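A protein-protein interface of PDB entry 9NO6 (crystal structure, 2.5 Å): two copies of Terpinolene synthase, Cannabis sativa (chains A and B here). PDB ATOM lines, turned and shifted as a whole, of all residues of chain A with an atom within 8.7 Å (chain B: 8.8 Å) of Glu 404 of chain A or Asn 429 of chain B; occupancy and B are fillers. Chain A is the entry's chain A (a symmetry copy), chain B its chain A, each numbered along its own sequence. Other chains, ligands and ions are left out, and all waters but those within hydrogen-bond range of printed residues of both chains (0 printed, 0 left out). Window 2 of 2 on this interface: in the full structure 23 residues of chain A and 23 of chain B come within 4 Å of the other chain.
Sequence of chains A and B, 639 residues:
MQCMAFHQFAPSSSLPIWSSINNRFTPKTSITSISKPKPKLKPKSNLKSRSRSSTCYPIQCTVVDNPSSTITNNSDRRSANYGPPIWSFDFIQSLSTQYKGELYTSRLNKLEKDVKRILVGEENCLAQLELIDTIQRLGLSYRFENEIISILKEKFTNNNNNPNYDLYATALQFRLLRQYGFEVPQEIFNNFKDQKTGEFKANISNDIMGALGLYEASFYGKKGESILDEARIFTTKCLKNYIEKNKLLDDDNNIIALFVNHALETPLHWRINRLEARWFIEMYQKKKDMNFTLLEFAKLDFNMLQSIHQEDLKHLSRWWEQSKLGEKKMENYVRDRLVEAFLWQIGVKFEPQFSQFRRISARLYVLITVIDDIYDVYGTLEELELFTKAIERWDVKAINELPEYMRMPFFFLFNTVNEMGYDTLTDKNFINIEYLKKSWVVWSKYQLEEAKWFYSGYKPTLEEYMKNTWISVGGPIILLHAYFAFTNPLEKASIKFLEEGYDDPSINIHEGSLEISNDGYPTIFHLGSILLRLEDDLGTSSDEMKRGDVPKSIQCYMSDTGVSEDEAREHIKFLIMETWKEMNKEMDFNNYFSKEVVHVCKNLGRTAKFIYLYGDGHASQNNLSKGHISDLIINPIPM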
ATOM      1  N   LYS A 324     -19.967 -30.826 -26.461  1.00  0.00           N
ATOM      2  CA  LYS A 324     -18.536 -30.521 -26.531  1.00  0.00           C
ATOM      3  C   LYS A 324     -17.719 -31.422 -25.610  1.00  0.00           C
ATOM      4  O   LYS A 324     -16.628 -31.055 -25.168  1.00  0.00           O
ATOM      5  CB  LYS A 324     -18.256 -29.045 -26.228  1.00  0.00           C
ATOM      6  CG  LYS A 324     -18.585 -28.090 -27.370  1.00  0.00           C
ATOM      7  CD  LYS A 324     -18.116 -26.664 -27.081  1.00  0.00           C
ATOM      8  CE  LYS A 324     -16.689 -26.421 -27.559  1.00  0.00           C
ATOM      9  NZ  LYS A 324     -16.229 -25.034 -27.254  1.00  0.00           N
ATOM     10  N   GLU A 383     -11.677 -37.771  -5.761  1.00  0.00           N
ATOM     11  CA  GLU A 383     -12.507 -37.184  -6.805  1.00  0.00           C
ATOM     12  C   GLU A 383     -13.785 -37.983  -7.024  1.00  0.00           C
ATOM     13  O   GLU A 383     -14.836 -37.402  -7.308  1.00  0.00           O
ATOM     14  CB  GLU A 383     -11.709 -37.084  -8.103  1.00  0.00           C
ATOM     15  CG  GLU A 383     -10.411 -36.305  -7.970  1.00  0.00           C
ATOM     16  CD  GLU A 383      -9.458 -36.566  -9.118  1.00  0.00           C
ATOM     17  OE1 GLU A 383      -9.732 -37.485  -9.920  1.00  0.00           O
ATOM     18  OE2 GLU A 383      -8.437 -35.857  -9.218  1.00  0.00           O
ATOM     19  N   LEU A 386     -16.154 -37.104  -4.292  1.00  0.00           N
ATOM     20  CA  LEU A 386     -16.731 -35.797  -4.600  1.00  0.00           C
ATOM     21  C   LEU A 386     -17.813 -35.907  -5.668  1.00  0.00           C
ATOM     22  O   LEU A 386     -18.881 -35.296  -5.545  1.00  0.00           O
ATOM     23  CB  LEU A 386     -15.634 -34.831  -5.048  1.00  0.00           C
ATOM     24  CG  LEU A 386     -14.559 -34.483  -4.017  1.00  0.00           C
ATOM     25  CD1 LEU A 386     -13.507 -33.572  -4.629  1.00  0.00           C
ATOM     26  CD2 LEU A 386     -15.183 -33.840  -2.790  1.00  0.00           C
ATOM     27  N   ILE A 399     -21.013 -27.730  -8.186  1.00  0.00           N
ATOM     28  CA  ILE A 399     -20.066 -27.866  -9.287  1.00  0.00           C
ATOM     29  C   ILE A 399     -18.730 -27.190  -8.980  1.00  0.00           C
ATOM     30  O   ILE A 399     -17.691 -27.614  -9.496  1.00  0.00           O
ATOM     31  CB  ILE A 399     -20.707 -27.316 -10.574  1.00  0.00           C
ATOM     32  CG1 ILE A 399     -21.995 -28.083 -10.878  1.00  0.00           C
ATOM     33  CG2 ILE A 399     -19.758 -27.416 -11.755  1.00  0.00           C
ATOM     34  CD1 ILE A 399     -22.649 -27.694 -12.180  1.00  0.00           C
ATOM     35  N   ASN A 400     -18.729 -26.155  -8.133  1.00  0.00           N
ATOM     36  CA  ASN A 400     -17.468 -25.579  -7.677  1.00  0.00           C
ATOM     37  C   ASN A 400     -16.619 -26.610  -6.945  1.00  0.00           C
ATOM     38  O   ASN A 400     -15.385 -26.563  -7.011  1.00  0.00           O
ATOM     39  CB  ASN A 400     -17.729 -24.382  -6.761  1.00  0.00           C
ATOM     40  CG  ASN A 400     -18.594 -23.325  -7.413  1.00  0.00           C
ATOM     41  OD1 ASN A 400     -19.822 -23.407  -7.384  1.00  0.00           O
ATOM     42  ND2 ASN A 400     -17.958 -22.316  -7.996  1.00  0.00           N
ATOM     43  N   GLU A 401     -17.262 -27.553  -6.253  1.00  0.00           N
ATOM     44  CA  GLU A 401     -16.538 -28.512  -5.427  1.00  0.00           C
ATOM     45  C   GLU A 401     -15.792 -29.543  -6.265  1.00  0.00           C
ATOM     46  O   GLU A 401     -14.772 -30.080  -5.818  1.00  0.00           O
ATOM     47  CB  GLU A 401     -17.511 -29.209  -4.478  1.00  0.00           C
ATOM     48  CG  GLU A 401     -18.363 -28.255  -3.655  1.00  0.00           C
ATOM     49  CD  GLU A 401     -19.568 -28.934  -3.030  1.00  0.00           C
ATOM     50  OE1 GLU A 401     -20.168 -29.809  -3.689  1.00  0.00           O
ATOM     51  OE2 GLU A 401     -19.914 -28.593  -1.879  1.00  0.00           O
ATOM     52  N   LEU A 402     -16.277 -29.832  -7.467  1.00  0.00           N
ATOM     53  CA  LEU A 402     -15.676 -30.872  -8.285  1.00  0.00           C
ATOM     54  C   LEU A 402     -14.398 -30.371  -8.954  1.00  0.00           C
ATOM     55  O   LEU A 402     -14.278 -29.183  -9.270  1.00  0.00           O
ATOM     56  CB  LEU A 402     -16.658 -31.340  -9.352  1.00  0.00           C
ATOM     57  CG  LEU A 402     -18.019 -31.815  -8.846  1.00  0.00           C
ATOM     58  CD1 LEU A 402     -18.966 -32.051 -10.007  1.00  0.00           C
ATOM     59  CD2 LEU A 402     -17.861 -33.074  -8.012  1.00  0.00           C
ATOM     60  N   PRO A 403     -13.426 -31.255  -9.173  1.00  0.00           N
ATOM     61  CA  PRO A 403     -12.250 -30.876  -9.964  1.00  0.00           C
ATOM     62  C   PRO A 403     -12.648 -30.471 -11.375  1.00  0.00           C
ATOM     63  O   PRO A 403     -13.731 -30.802 -11.864  1.00  0.00           O
ATOM     64  CB  PRO A 403     -11.387 -32.146  -9.962  1.00  0.00           C
ATOM     65  CG  PRO A 403     -12.310 -33.250  -9.547  1.00  0.00           C
ATOM     66  CD  PRO A 403     -13.317 -32.623  -8.639  1.00  0.00           C
ATOM     67  N   GLU A 404     -11.738 -29.747 -12.034  1.00  0.00           N
ATOM     68  CA  GLU A 404     -12.075 -29.071 -13.285  1.00  0.00           C
ATOM     69  C   GLU A 404     -12.585 -30.046 -14.340  1.00  0.00           C
ATOM     70  O   GLU A 404     -13.557 -29.751 -15.046  1.00  0.00           O
ATOM     71  CB  GLU A 404     -10.861 -28.301 -13.804  1.00  0.00           C
ATOM     72  CG  GLU A 404     -11.093 -27.592 -15.131  1.00  0.00           C
ATOM     73  CD  GLU A 404     -10.398 -28.284 -16.288  1.00  0.00           C
ATOM     74  OE1 GLU A 404      -9.414 -29.011 -16.040  1.00  0.00           O
ATOM     75  OE2 GLU A 404     -10.836 -28.101 -17.443  1.00  0.00           O
ATOM     76  N   TYR A 405     -11.954 -31.215 -14.460  1.00  0.00           N
ATOM     77  CA  TYR A 405     -12.355 -32.154 -15.500  1.00  0.00           C
ATOM     78  C   TYR A 405     -13.663 -32.868 -15.183  1.00  0.00           C
ATOM     79  O   TYR A 405     -14.231 -33.504 -16.077  1.00  0.00           O
ATOM     80  CB  TYR A 405     -11.246 -33.180 -15.743  1.00  0.00           C
ATOM     81  CG  TYR A 405     -11.239 -34.341 -14.774  1.00  0.00           C
ATOM     82  CD1 TYR A 405     -10.668 -34.218 -13.514  1.00  0.00           C
ATOM     83  CD2 TYR A 405     -11.789 -35.568 -15.127  1.00  0.00           C
ATOM     84  CE1 TYR A 405     -10.655 -35.280 -12.630  1.00  0.00           C
ATOM     85  CE2 TYR A 405     -11.781 -36.635 -14.250  1.00  0.00           C
ATOM     86  CZ  TYR A 405     -11.214 -36.487 -13.004  1.00  0.00           C
ATOM     87  OH  TYR A 405     -11.204 -37.547 -12.128  1.00  0.00           O
ATOM     88  N   MET A 406     -14.153 -32.778 -13.945  1.00  0.00           N
ATOM     89  CA  MET A 406     -15.401 -33.423 -13.556  1.00  0.00           C
ATOM     90  C   MET A 406     -16.613 -32.505 -13.631  1.00  0.00           C
ATOM     91  O   MET A 406     -17.740 -33.006 -13.710  1.00  0.00           O
ATOM     92  CB  MET A 406     -15.293 -33.977 -12.131  1.00  0.00           C
ATOM     93  CG  MET A 406     -14.720 -35.381 -12.037  1.00  0.00           C
ATOM     94  SD  MET A 406     -14.550 -35.918 -10.324  1.00  0.00           S
ATOM     95  CE  MET A 406     -14.259 -37.670 -10.536  1.00  0.00           C
ATOM     96  N   ARG A 407     -16.412 -31.184 -13.599  1.00  0.00           N
ATOM     97  CA  ARG A 407     -17.539 -30.254 -13.632  1.00  0.00           C
ATOM     98  C   ARG A 407     -18.378 -30.456 -14.886  1.00  0.00           C
ATOM     99  O   ARG A 407     -19.606 -30.586 -14.817  1.00  0.00           O
ATOM    100  CB  ARG A 407     -17.037 -28.813 -13.579  1.00  0.00           C
ATOM    101  CG  ARG A 407     -15.802 -28.587 -12.739  1.00  0.00           C
ATOM    102  CD  ARG A 407     -15.302 -27.165 -12.923  1.00  0.00           C
ATOM    103  NE  ARG A 407     -14.182 -26.858 -12.044  1.00  0.00           N
ATOM    104  CZ  ARG A 407     -14.308 -26.520 -10.769  1.00  0.00           C
ATOM    105  NH1 ARG A 407     -15.492 -26.456 -10.184  1.00  0.00           N
ATOM    106  NH2 ARG A 407     -13.217 -26.242 -10.061  1.00  0.00           N
ATOM    107  N   MET A 408     -17.721 -30.478 -16.041  1.00  0.00           N
ATOM    108  CA  MET A 408     -18.426 -30.553 -17.318  1.00  0.00           C
ATOM    109  C   MET A 408     -19.270 -31.816 -17.455  1.00  0.00           C
ATOM    110  O   MET A 408     -20.463 -31.697 -17.792  1.00  0.00           O
ATOM    111  CB  MET A 408     -17.397 -30.416 -18.444  1.00  0.00           C
ATOM    112  CG  MET A 408     -17.906 -29.852 -19.743  1.00  0.00           C
ATOM    113  SD  MET A 408     -16.498 -29.608 -20.839  1.00  0.00           S
ATOM    114  CE  MET A 408     -17.318 -29.371 -22.405  1.00  0.00           C
ATOM    115  N   PRO A 409     -18.752 -33.030 -17.213  1.00  0.00           N
ATOM    116  CA  PRO A 409     -19.632 -34.208 -17.305  1.00  0.00           C
ATOM    117  C   PRO A 409     -20.748 -34.211 -16.274  1.00  0.00           C
ATOM    118  O   PRO A 409     -21.876 -34.597 -16.604  1.00  0.00           O
ATOM    119  CB  PRO A 409     -18.664 -35.386 -17.109  1.00  0.00           C
ATOM    120  CG  PRO A 409     -17.496 -34.807 -16.404  1.00  0.00           C
ATOM    121  CD  PRO A 409     -17.357 -33.423 -16.938  1.00  0.00           C
ATOM    122  N   PHE A 410     -20.475 -33.788 -15.037  1.00  0.00           N
ATOM    123  CA  PHE A 410     -21.543 -33.728 -14.043  1.00  0.00           C
ATOM    124  C   PHE A 410     -22.600 -32.704 -14.427  1.00  0.00           C
ATOM    125  O   PHE A 410     -23.799 -32.966 -14.292  1.00  0.00           O
ATOM    126  CB  PHE A 410     -20.989 -33.404 -12.657  1.00  0.00           C
ATOM    127  CG  PHE A 410     -22.059 -33.066 -11.650  1.00  0.00           C
ATOM    128  CD1 PHE A 410     -22.735 -34.070 -10.977  1.00  0.00           C
ATOM    129  CD2 PHE A 410     -22.399 -31.747 -11.391  1.00  0.00           C
ATOM    130  CE1 PHE A 410     -23.725 -33.766 -10.060  1.00  0.00           C
ATOM    131  CE2 PHE A 410     -23.390 -31.438 -10.478  1.00  0.00           C
ATOM    132  CZ  PHE A 410     -24.052 -32.447  -9.810  1.00  0.00           C
ATOM    133  N   GLY B 421     -25.880 -21.787 -18.568  1.00  0.00           N
ATOM    134  CA  GLY B 421     -24.697 -21.899 -17.730  1.00  0.00           C
ATOM    135  C   GLY B 421     -23.739 -22.966 -18.224  1.00  0.00           C
ATOM    136  O   GLY B 421     -22.518 -22.784 -18.195  1.00  0.00           O
ATOM    137  N   TYR B 422     -24.280 -24.092 -18.696  1.00  0.00           N
ATOM    138  CA  TYR B 422     -23.426 -25.126 -19.269  1.00  0.00           C
ATOM    139  C   TYR B 422     -22.786 -24.655 -20.567  1.00  0.00           C
ATOM    140  O   TYR B 422     -21.641 -25.011 -20.860  1.00  0.00           O
ATOM    141  CB  TYR B 422     -24.220 -26.410 -19.509  1.00  0.00           C
ATOM    142  CG  TYR B 422     -23.374 -27.519 -20.091  1.00  0.00           C
ATOM    143  CD1 TYR B 422     -22.600 -28.328 -19.269  1.00  0.00           C
ATOM    144  CD2 TYR B 422     -23.334 -27.750 -21.460  1.00  0.00           C
ATOM    145  CE1 TYR B 422     -21.819 -29.339 -19.791  1.00  0.00           C
ATOM    146  CE2 TYR B 422     -22.554 -28.759 -21.993  1.00  0.00           C
ATOM    147  CZ  TYR B 422     -21.799 -29.551 -21.153  1.00  0.00           C
ATOM    148  OH  TYR B 422     -21.019 -30.558 -21.673  1.00  0.00           O
ATOM    149  N   ASP B 423     -23.517 -23.875 -21.367  1.00  0.00           N
ATOM    150  CA  ASP B 423     -22.926 -23.293 -22.568  1.00  0.00           C
ATOM    151  C   ASP B 423     -21.726 -22.428 -22.216  1.00  0.00           C
ATOM    152  O   ASP B 423     -20.693 -22.473 -22.897  1.00  0.00           O
ATOM    153  CB  ASP B 423     -23.969 -22.476 -23.333  1.00  0.00           C
ATOM    154  CG  ASP B 423     -24.897 -23.341 -24.158  1.00  0.00           C
ATOM    155  OD1 ASP B 423     -24.467 -24.430 -24.596  1.00  0.00           O
ATOM    156  OD2 ASP B 423     -26.057 -22.931 -24.375  1.00  0.00           O
ATOM    157  N   THR B 424     -21.839 -21.639 -21.149  1.00  0.00           N
ATOM    158  CA  THR B 424     -20.690 -20.845 -20.718  1.00  0.00           C
ATOM    159  C   THR B 424     -19.551 -21.737 -20.232  1.00  0.00           C
ATOM    160  O   THR B 424     -18.387 -21.513 -20.588  1.00  0.00           O
ATOM    161  CB  THR B 424     -21.096 -19.854 -19.630  1.00  0.00           C
ATOM    162  OG1 THR B 424     -21.954 -18.855 -20.193  1.00  0.00           O
ATOM    163  CG2 THR B 424     -19.863 -19.179 -19.044  1.00  0.00           C
ATOM    164  N   LEU B 425     -19.865 -22.760 -19.430  1.00  0.00           N
ATOM    165  CA  LEU B 425     -18.820 -23.656 -18.934  1.00  0.00           C
ATOM    166  C   LEU B 425     -18.100 -24.374 -20.070  1.00  0.00           C
ATOM    167  O   LEU B 425     -16.897 -24.640 -19.972  1.00  0.00           O
ATOM    168  CB  LEU B 425     -19.410 -24.675 -17.956  1.00  0.00           C
ATOM    169  CG  LEU B 425     -18.458 -25.759 -17.432  1.00  0.00           C
ATOM    170  CD1 LEU B 425     -17.251 -25.139 -16.743  1.00  0.00           C
ATOM    171  CD2 LEU B 425     -19.172 -26.719 -16.492  1.00  0.00           C
ATOM    172  N   THR B 426     -18.810 -24.686 -21.153  1.00  0.00           N
ATOM    173  CA  THR B 426     -18.213 -25.442 -22.246  1.00  0.00           C
ATOM    174  C   THR B 426     -17.516 -24.560 -23.273  1.00  0.00           C
ATOM    175  O   THR B 426     -16.562 -25.014 -23.917  1.00  0.00           O
ATOM    176  CB  THR B 426     -19.273 -26.302 -22.946  1.00  0.00           C
ATOM    177  OG1 THR B 426     -18.641 -27.104 -23.945  1.00  0.00           O
ATOM    178  CG2 THR B 426     -20.311 -25.447 -23.630  1.00  0.00           C
ATOM    179  N   ASP B 427     -17.952 -23.310 -23.441  1.00  0.00           N
ATOM    180  CA  ASP B 427     -17.339 -22.439 -24.432  1.00  0.00           C
ATOM    181  C   ASP B 427     -16.247 -21.549 -23.858  1.00  0.00           C
ATOM    182  O   ASP B 427     -15.376 -21.101 -24.611  1.00  0.00           O
ATOM    183  CB  ASP B 427     -18.408 -21.565 -25.097  1.00  0.00           C
ATOM    184  CG  ASP B 427     -19.450 -22.382 -25.840  1.00  0.00           C
ATOM    185  OD1 ASP B 427     -19.078 -23.400 -26.462  1.00  0.00           O
ATOM    186  OD2 ASP B 427     -20.640 -22.006 -25.801  1.00  0.00           O
ATOM    187  N   LYS B 428     -16.265 -21.285 -22.547  1.00  0.00           N
ATOM    188  CA  LYS B 428     -15.310 -20.359 -21.955  1.00  0.00           C
ATOM    189  C   LYS B 428     -14.739 -20.851 -20.629  1.00  0.00           C
ATOM    190  O   LYS B 428     -14.093 -20.063 -19.928  1.00  0.00           O
ATOM    191  CB  LYS B 428     -15.957 -18.980 -21.750  1.00  0.00           C
ATOM    192  CG  LYS B 428     -16.329 -18.260 -23.040  1.00  0.00           C
ATOM    193  CD  LYS B 428     -16.899 -16.880 -22.754  1.00  0.00           C
ATOM    194  CE  LYS B 428     -17.007 -16.042 -24.018  1.00  0.00           C
ATOM    195  NZ  LYS B 428     -17.997 -16.591 -24.983  1.00  0.00           N
ATOM    196  N   ASN B 429     -14.955 -22.119 -20.268  1.00  0.00           N
ATOM    197  CA  ASN B 429     -14.454 -22.708 -19.027  1.00  0.00           C
ATOM    198  C   ASN B 429     -14.675 -21.783 -17.836  1.00  0.00           C
ATOM    199  O   ASN B 429     -13.717 -21.288 -17.233  1.00  0.00           O
ATOM    200  CB  ASN B 429     -12.971 -23.063 -19.159  1.00  0.00           C
ATOM    201  CG  ASN B 429     -12.550 -24.168 -18.204  1.00  0.00           C
ATOM    202  OD1 ASN B 429     -13.378 -24.957 -17.747  1.00  0.00           O
ATOM    203  ND2 ASN B 429     -11.259 -24.229 -17.902  1.00  0.00           N
ATOM    204  N   PHE B 430     -15.939 -21.541 -17.500  1.00  0.00           N
ATOM    205  CA  PHE B 430     -16.294 -20.625 -16.428  1.00  0.00           C
ATOM    206  C   PHE B 430     -17.673 -21.004 -15.910  1.00  0.00           C
ATOM    207  O   PHE B 430     -18.563 -21.342 -16.693  1.00  0.00           O
ATOM    208  CB  PHE B 430     -16.279 -19.173 -16.918  1.00  0.00           C
ATOM    209  CG  PHE B 430     -16.593 -18.163 -15.852  1.00  0.00           C
ATOM    210  CD1 PHE B 430     -15.597 -17.684 -15.017  1.00  0.00           C
ATOM    211  CD2 PHE B 430     -17.881 -17.679 -15.694  1.00  0.00           C
ATOM    212  CE1 PHE B 430     -15.883 -16.751 -14.039  1.00  0.00           C
ATOM    213  CE2 PHE B 430     -18.171 -16.745 -14.719  1.00  0.00           C
ATOM    214  CZ  PHE B 430     -17.172 -16.281 -13.891  1.00  0.00           C
ATOM    215  N   ILE B 431     -17.837 -20.947 -14.593  1.00  0.00           N
ATOM    216  CA  ILE B 431     -19.088 -21.308 -13.938  1.00  0.00           C
ATOM    217  C   ILE B 431     -19.804 -20.005 -13.604  1.00  0.00           C
ATOM    218  O   ILE B 431     -19.477 -19.332 -12.622  1.00  0.00           O
ATOM    219  CB  ILE B 431     -18.856 -22.166 -12.691  1.00  0.00           C
ATOM    220  CG1 ILE B 431     -17.977 -23.377 -13.021  1.00  0.00           C
ATOM    221  CG2 ILE B 431     -20.183 -22.628 -12.112  1.00  0.00           C
ATOM    222  CD1 ILE B 431     -16.500 -23.179 -12.716  1.00  0.00           C
ATOM    223  N   ASN B 432     -20.787 -19.644 -14.425  1.00  0.00           N
ATOM    224  CA  ASN B 432     -21.548 -18.416 -14.247  1.00  0.00           C
ATOM    225  C   ASN B 432     -22.980 -18.664 -13.800  1.00  0.00           C
ATOM    226  O   ASN B 432     -23.758 -17.708 -13.709  1.00  0.00           O
ATOM    227  CB  ASN B 432     -21.549 -17.603 -15.545  1.00  0.00           C
ATOM    228  CG  ASN B 432     -22.238 -18.328 -16.685  1.00  0.00           C
ATOM    229  OD1 ASN B 432     -22.468 -19.537 -16.620  1.00  0.00           O
ATOM    230  ND2 ASN B 432     -22.564 -17.596 -17.742  1.00  0.00           N
ATOM    231  N   PHE B 484     -21.721 -12.584 -20.671  1.00  0.00           N
ATOM    232  CA  PHE B 484     -21.037 -13.873 -20.651  1.00  0.00           C
ATOM    233  C   PHE B 484     -20.896 -14.478 -22.042  1.00  0.00           C
ATOM    234  O   PHE B 484     -20.086 -15.394 -22.227  1.00  0.00           O
ATOM    235  CB  PHE B 484     -21.761 -14.836 -19.714  1.00  0.00           C
ATOM    236  CG  PHE B 484     -21.572 -14.510 -18.264  1.00  0.00           C
ATOM    237  CD1 PHE B 484     -20.317 -14.179 -17.779  1.00  0.00           C
ATOM    238  CD2 PHE B 484     -22.645 -14.504 -17.392  1.00  0.00           C
ATOM    239  CE1 PHE B 484     -20.134 -13.867 -16.447  1.00  0.00           C
ATOM    240  CE2 PHE B 484     -22.468 -14.195 -16.058  1.00  0.00           C
ATOM    241  CZ  PHE B 484     -21.211 -13.873 -15.585  1.00  0.00           C
ATOM    242  N   ASN B 488     -14.626 -12.566 -22.262  1.00  0.00           N
ATOM    243  CA  ASN B 488     -13.823 -13.635 -21.689  1.00  0.00           C
ATOM    244  C   ASN B 488     -13.842 -13.523 -20.171  1.00  0.00           C
ATOM    245  O   ASN B 488     -13.298 -12.551 -19.629  1.00  0.00           O
ATOM    246  CB  ASN B 488     -12.391 -13.563 -22.213  1.00  0.00           C
ATOM    247  CG  ASN B 488     -11.575 -14.778 -21.836  1.00  0.00           C
ATOM    248  OD1 ASN B 488     -12.125 -15.845 -21.571  1.00  0.00           O
ATOM    249  ND2 ASN B 488     -10.256 -14.626 -21.812  1.00  0.00           N
ATOM    250  N   PRO B 489     -14.449 -14.466 -19.447  1.00  0.00           N
ATOM    251  CA  PRO B 489     -14.565 -14.319 -17.991  1.00  0.00           C
ATOM    252  C   PRO B 489     -13.350 -14.799 -17.215  1.00  0.00           C
ATOM    253  O   PRO B 489     -13.300 -14.590 -15.995  1.00  0.00           O
ATOM    254  CB  PRO B 489     -15.798 -15.167 -17.660  1.00  0.00           C
ATOM    255  CG  PRO B 489     -15.779 -16.238 -18.692  1.00  0.00           C
ATOM    256  CD  PRO B 489     -15.145 -15.669 -19.936  1.00  0.00           C
ATOM    257  N   LEU B 490     -12.377 -15.433 -17.869  1.00  0.00           N
ATOM    258  CA  LEU B 490     -11.132 -15.792 -17.201  1.00  0.00           C
ATOM    259  C   LEU B 490     -10.169 -14.617 -17.091  1.00  0.00           C
ATOM    260  O   LEU B 490      -9.062 -14.791 -16.571  1.00  0.00           O
ATOM    261  CB  LEU B 490     -10.443 -16.947 -17.931  1.00  0.00           C
ATOM    262  CG  LEU B 490     -11.257 -18.210 -18.202  1.00  0.00           C
ATOM    263  CD1 LEU B 490     -11.626 -18.271 -19.667  1.00  0.00           C
ATOM    264  CD2 LEU B 490     -10.481 -19.450 -17.795  1.00  0.00           C
ATOM    265  N   GLU B 491     -10.559 -13.440 -17.570  1.00  0.00           N
ATOM    266  CA  GLU B 491      -9.718 -12.260 -17.486  1.00  0.00           C
ATOM    267  C   GLU B 491      -9.828 -11.624 -16.102  1.00  0.00           C
ATOM    268  O   GLU B 491     -10.687 -11.974 -15.289  1.00  0.00           O
ATOM    269  CB  GLU B 491     -10.098 -11.256 -18.572  1.00  0.00           C
ATOM    270  CG  GLU B 491      -9.809 -11.740 -19.984  1.00  0.00           C
ATOM    271  CD  GLU B 491     -10.452 -10.867 -21.044  1.00  0.00           C
ATOM    272  OE1 GLU B 491     -11.358 -10.080 -20.700  1.00  0.00           O
ATOM    273  OE2 GLU B 491     -10.053 -10.970 -22.224  1.00  0.00           O
ATOM    274  N   ILE B 495     -13.326 -11.135 -13.509  1.00  0.00           N
ATOM    275  CA  ILE B 495     -13.304 -11.689 -12.158  1.00  0.00           C
ATOM    276  C   ILE B 495     -13.411 -10.584 -11.117  1.00  0.00           C
ATOM    277  O   ILE B 495     -14.042 -10.765 -10.068  1.00  0.00           O
ATOM    278  CB  ILE B 495     -12.033 -12.543 -11.962  1.00  0.00           C
ATOM    279  CG1 ILE B 495     -12.056 -13.744 -12.911  1.00  0.00           C
ATOM    280  CG2 ILE B 495     -11.905 -13.006 -10.519  1.00  0.00           C
ATOM    281  CD1 ILE B 495     -10.835 -14.631 -12.806  1.00  0.00           C
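Hydrophobic or aromatic side chains of chain B within 4 Å of the printed part of chain A: Tyr 422 and Leu 425. Of the 15 printed residues of chain A, 3 touch a printed residue of chain B. Hydrophobic or aromatic side chains of chain A that line the printed part of chain B: Met 408. Among the printed residues, Asp or Glu carboxylates within 4 Å of a Lys or Arg side-chain nitrogen of the other chain: Lys 324 of chain A with Asp 427 of chain B.
The backbone NH (N) of Leu 425 of chain B sits close to the backbone carbonyl oxygen (O) of Phe 430 of chain B, at 3.3 Å.
No position is printed for both chains.
NZ of Lys 324 of chain A is in hydrogen-bond range of O of Thr 426 of chain B, at 3.4 Å. The side-chain carboxylate of Asp 427 of chain B lies within salt-bridge range of the side-chain amino group of Lys 324 of chain A (3.4 Å).
Glu 404 of chain A touches just one residue of chain B: Asn 429 (3.9 Å). Of the printed residues of chain A, Asn 429 of chain B touches Glu 404 (3.9 Å). Of the printed residues of chain A, Asp 427 of chain B touches Lys 324. Printed residues of chain A within 4 Å of Thr 426 of chain B: Lys 324 (3.0 Å) and Met 408 (3.0 Å). Printed residues of chain B within 4 Å of Lys 324 of chain A: Thr 426 (3.0 Å) and Asp 427 (3.4 Å). Of the printed residues of chain A, Leu 425 of chain B touches Met 408 (3.99 Å). Pro 489 of chain B touches none of the printed residues of chain A. Leu 490 of chain B touches none of the printed residues of chain A. The nearest residue of chain B that does not touch Glu 404 of chain A is Leu 425 of chain B (6.1 Å). The nearest residue of chain A that does not touch Asn 429 of chain B is Arg 407 of chain A (5.6 Å). The nearest printed residue of chain A that does not touch Tyr 422 of chain B is Lys 324 of chain A (4.9 Å).
Among the printed residues, pairs that only touch across the chains: Glu 404 of chain A with Asn 429 of chain B, Met 408 of chain A with Tyr 422 of chain B, Met 408 of chain A with Leu 425 of chain B and Met 408 of chain A with Thr 426 of chain B.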
